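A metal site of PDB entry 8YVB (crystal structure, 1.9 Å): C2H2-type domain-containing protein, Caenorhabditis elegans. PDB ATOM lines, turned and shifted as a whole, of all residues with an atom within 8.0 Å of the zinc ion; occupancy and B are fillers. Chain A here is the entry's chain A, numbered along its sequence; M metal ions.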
ATOM      1  N   LYS A  63      16.780  -8.866 -16.989  1.00  0.00           N
ATOM      2  CA  LYS A  63      16.919  -9.876 -15.941  1.00  0.00           C
ATOM      3  C   LYS A  63      18.348  -9.897 -15.430  1.00  0.00           C
ATOM      4  O   LYS A  63      19.300  -9.832 -16.215  1.00  0.00           O
ATOM      5  CB  LYS A  63      16.532 -11.261 -16.469  1.00  0.00           C
ATOM      6  CG  LYS A  63      15.112 -11.336 -17.018  1.00  0.00           C
ATOM      7  CD  LYS A  63      14.747 -12.752 -17.403  1.00  0.00           C
ATOM      8  CE  LYS A  63      13.377 -12.819 -18.076  1.00  0.00           C
ATOM      9  NZ  LYS A  63      13.367 -12.079 -19.377  1.00  0.00           N
ATOM     10  N   CYS A  64      18.504  -9.965 -14.115  1.00  0.00           N
ATOM     11  CA  CYS A  64      19.834 -10.082 -13.534  1.00  0.00           C
ATOM     12  C   CYS A  64      20.379 -11.480 -13.780  1.00  0.00           C
ATOM     13  O   CYS A  64      19.677 -12.481 -13.569  1.00  0.00           O
ATOM     14  CB  CYS A  64      19.800  -9.776 -12.043  1.00  0.00           C
ATOM     15  SG  CYS A  64      21.416  -9.870 -11.235  1.00  0.00           S
ATOM     16  N   ASN A  65      21.626 -11.569 -14.240  1.00  0.00           N
ATOM     17  CA  ASN A  65      22.249 -12.864 -14.487  1.00  0.00           C
ATOM     18  C   ASN A  65      22.758 -13.537 -13.219  1.00  0.00           C
ATOM     19  O   ASN A  65      23.284 -14.638 -13.300  1.00  0.00           O
ATOM     20  CB  ASN A  65      23.409 -12.703 -15.483  1.00  0.00           C
ATOM     21  CG  ASN A  65      22.955 -12.218 -16.841  1.00  0.00           C
ATOM     22  OD1 ASN A  65      21.903 -12.630 -17.331  1.00  0.00           O
ATOM     23  ND2 ASN A  65      23.735 -11.348 -17.454  1.00  0.00           N
ATOM     24  N   PHE A  66      22.595 -12.892 -12.061  1.00  0.00           N
ATOM     25  CA  PHE A  66      23.113 -13.423 -10.806  1.00  0.00           C
ATOM     26  C   PHE A  66      22.051 -13.666  -9.753  1.00  0.00           C
ATOM     27  O   PHE A  66      22.364 -14.240  -8.702  1.00  0.00           O
ATOM     28  CB  PHE A  66      24.180 -12.475 -10.230  1.00  0.00           C
ATOM     29  CG  PHE A  66      25.282 -12.159 -11.200  1.00  0.00           C
ATOM     30  CD1 PHE A  66      26.340 -13.033 -11.378  1.00  0.00           C
ATOM     31  CD2 PHE A  66      25.245 -10.981 -11.940  1.00  0.00           C
ATOM     32  CE1 PHE A  66      27.349 -12.739 -12.281  1.00  0.00           C
ATOM     33  CE2 PHE A  66      26.254 -10.687 -12.843  1.00  0.00           C
ATOM     34  CZ  PHE A  66      27.303 -11.563 -13.011  1.00  0.00           C
ATOM     35  N   CYS A  67      20.812 -13.243  -9.986  1.00  0.00           N
ATOM     36  CA  CYS A  67      19.695 -13.559  -9.092  1.00  0.00           C
ATOM     37  C   CYS A  67      18.404 -13.398  -9.891  1.00  0.00           C
ATOM     38  O   CYS A  67      18.427 -13.144 -11.102  1.00  0.00           O
ATOM     39  CB  CYS A  67      19.702 -12.681  -7.838  1.00  0.00           C
ATOM     40  SG  CYS A  67      19.288 -10.943  -8.099  1.00  0.00           S
ATOM     41  N   ASP A  68      17.283 -13.558  -9.205  1.00  0.00           N
ATOM     42  CA  ASP A  68      15.981 -13.473  -9.869  1.00  0.00           C
ATOM     43  C   ASP A  68      15.492 -12.045 -10.042  1.00  0.00           C
ATOM     44  O   ASP A  68      14.334 -11.850 -10.441  1.00  0.00           O
ATOM     45  CB  ASP A  68      14.942 -14.288  -9.090  1.00  0.00           C
ATOM     46  CG  ASP A  68      15.270 -15.767  -9.057  1.00  0.00           C
ATOM     47  OD1 ASP A  68      15.934 -16.215  -8.111  1.00  0.00           O
ATOM     48  OD2 ASP A  68      14.848 -16.485  -9.988  1.00  0.00           O
ATOM     49  N   TYR A  69      16.324 -11.043  -9.761  1.00  0.00           N
ATOM     50  CA  TYR A  69      15.909  -9.659  -9.909  1.00  0.00           C
ATOM     51  C   TYR A  69      15.634  -9.345 -11.379  1.00  0.00           C
ATOM     52  O   TYR A  69      16.353  -9.789 -12.278  1.00  0.00           O
ATOM     53  CB  TYR A  69      16.971  -8.714  -9.356  1.00  0.00           C
ATOM     54  CG  TYR A  69      16.640  -7.242  -9.521  1.00  0.00           C
ATOM     55  CD1 TYR A  69      15.815  -6.606  -8.603  1.00  0.00           C
ATOM     56  CD2 TYR A  69      17.141  -6.506 -10.579  1.00  0.00           C
ATOM     57  CE1 TYR A  69      15.507  -5.258  -8.734  1.00  0.00           C
ATOM     58  CE2 TYR A  69      16.842  -5.157 -10.722  1.00  0.00           C
ATOM     59  CZ  TYR A  69      16.024  -4.548  -9.802  1.00  0.00           C
ATOM     60  OH  TYR A  69      15.714  -3.208  -9.927  1.00  0.00           O
ATOM     61  N   MET A  70      14.583  -8.570 -11.610  1.00  0.00           N
ATOM     62  CA  MET A  70      14.240  -8.068 -12.929  1.00  0.00           C
ATOM     63  C   MET A  70      13.872  -6.607 -12.813  1.00  0.00           C
ATOM     64  O   MET A  70      13.354  -6.161 -11.787  1.00  0.00           O
ATOM     65  CB  MET A  70      13.098  -8.849 -13.574  1.00  0.00           C
ATOM     66  CG  MET A  70      13.398 -10.301 -13.864  1.00  0.00           C
ATOM     67  SD  MET A  70      12.001 -11.108 -14.677  1.00  0.00           S
ATOM     68  CE  MET A  70      10.702 -10.806 -13.485  1.00  0.00           C
ATOM     69  N   ILE A  77      19.485  -1.836 -14.366  1.00  0.00           N
ATOM     70  CA  ILE A  77      20.112  -3.145 -14.161  1.00  0.00           C
ATOM     71  C   ILE A  77      21.573  -2.980 -13.784  1.00  0.00           C
ATOM     72  O   ILE A  77      22.110  -3.778 -13.002  1.00  0.00           O
ATOM     73  CB  ILE A  77      19.933  -4.054 -15.395  1.00  0.00           C
ATOM     74  CG1 ILE A  77      20.235  -5.509 -15.029  1.00  0.00           C
ATOM     75  CG2 ILE A  77      20.827  -3.620 -16.543  1.00  0.00           C
ATOM     76  CD1 ILE A  77      19.298  -6.084 -13.968  1.00  0.00           C
ATOM     77  N   HIS A  80      21.588  -2.121 -10.157  1.00  0.00           N
ATOM     78  CA  HIS A  80      21.362  -3.339  -9.381  1.00  0.00           C
ATOM     79  C   HIS A  80      22.641  -4.153  -9.257  1.00  0.00           C
ATOM     80  O   HIS A  80      22.952  -4.668  -8.178  1.00  0.00           O
ATOM     81  CB  HIS A  80      20.263  -4.182 -10.038  1.00  0.00           C
ATOM     82  CG  HIS A  80      20.124  -5.546  -9.419  1.00  0.00           C
ATOM     83  ND1 HIS A  80      19.500  -5.743  -8.212  1.00  0.00           N
ATOM     84  CD2 HIS A  80      20.535  -6.761  -9.844  1.00  0.00           C
ATOM     85  CE1 HIS A  80      19.520  -7.035  -7.911  1.00  0.00           C
ATOM     86  NE2 HIS A  80      20.145  -7.670  -8.882  1.00  0.00           N
ATOM     87  N   HIS A  81      23.384  -4.299 -10.352  1.00  0.00           N
ATOM     88  CA  HIS A  81      24.646  -5.041 -10.313  1.00  0.00           C
ATOM     89  C   HIS A  81      25.619  -4.413  -9.325  1.00  0.00           C
ATOM     90  O   HIS A  81      26.237  -5.115  -8.515  1.00  0.00           O
ATOM     91  CB  HIS A  81      25.265  -5.097 -11.705  1.00  0.00           C
ATOM     92  CG  HIS A  81      24.568  -6.029 -12.649  1.00  0.00           C
ATOM     93  ND1 HIS A  81      24.568  -5.833 -14.016  1.00  0.00           N
ATOM     94  CD2 HIS A  81      23.859  -7.163 -12.429  1.00  0.00           C
ATOM     95  CE1 HIS A  81      23.876  -6.804 -14.593  1.00  0.00           C
ATOM     96  NE2 HIS A  81      23.440  -7.617 -13.661  1.00  0.00           N
ATOM     97  N   SER A  84      23.943  -4.818  -5.540  1.00  0.00           N
ATOM     98  CA  SER A  84      23.633  -6.146  -5.035  1.00  0.00           C
ATOM     99  C   SER A  84      24.726  -7.177  -5.322  1.00  0.00           C
ATOM    100  O   SER A  84      24.749  -8.208  -4.650  1.00  0.00           O
ATOM    101  CB  SER A  84      22.309  -6.651  -5.634  1.00  0.00           C
ATOM    102  OG  SER A  84      21.222  -5.875  -5.183  1.00  0.00           O
ATOM    103  N   HIS A  85      25.612  -6.927  -6.287  1.00  0.00           N
ATOM    104  CA  HIS A  85      26.644  -7.883  -6.657  1.00  0.00           C
ATOM    105  C   HIS A  85      28.009  -7.204  -6.778  1.00  0.00           C
ATOM    106  O   HIS A  85      28.647  -7.260  -7.832  1.00  0.00           O
ATOM    107  CB  HIS A  85      26.270  -8.584  -7.960  1.00  0.00           C
ATOM    108  CG  HIS A  85      24.880  -9.151  -7.961  1.00  0.00           C
ATOM    109  ND1 HIS A  85      24.565 -10.334  -7.315  1.00  0.00           N
ATOM    110  CD2 HIS A  85      23.730  -8.698  -8.510  1.00  0.00           C
ATOM    111  CE1 HIS A  85      23.276 -10.573  -7.472  1.00  0.00           C
ATOM    112  NE2 HIS A  85      22.748  -9.608  -8.199  1.00  0.00           N
HETATM  113 ZN    ZN M   1      20.885  -9.621  -9.091  1.00  0.00          ZN
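The zinc ion is bound by NE2 of His 85 (2.1 Å), NE2 of His 80 (2.1 Å), SG of Cys 64 (2.2 Å) and SG of Cys 67 (2.3 Å).
SG of Cys 64 sits close to N of Phe 66, 3.3 Å away. ND1 of His 80 sits close to OG of Ser 84, at 3.5 Å. O of Tyr 69 lies within hydrogen-bond range of N of Cys 64, at 2.8 Å. The backbone NH (N) of Tyr 69 lies close to the side-chain sulfur (SG) of Cys 67, 3.4 Å away.
Within 4 Å of the zinc ion: Cys 64, Cys 67, His 80 and His 85. The nearest printed residue that does not touch the zinc ion is Tyr 69 (4.03 Å).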
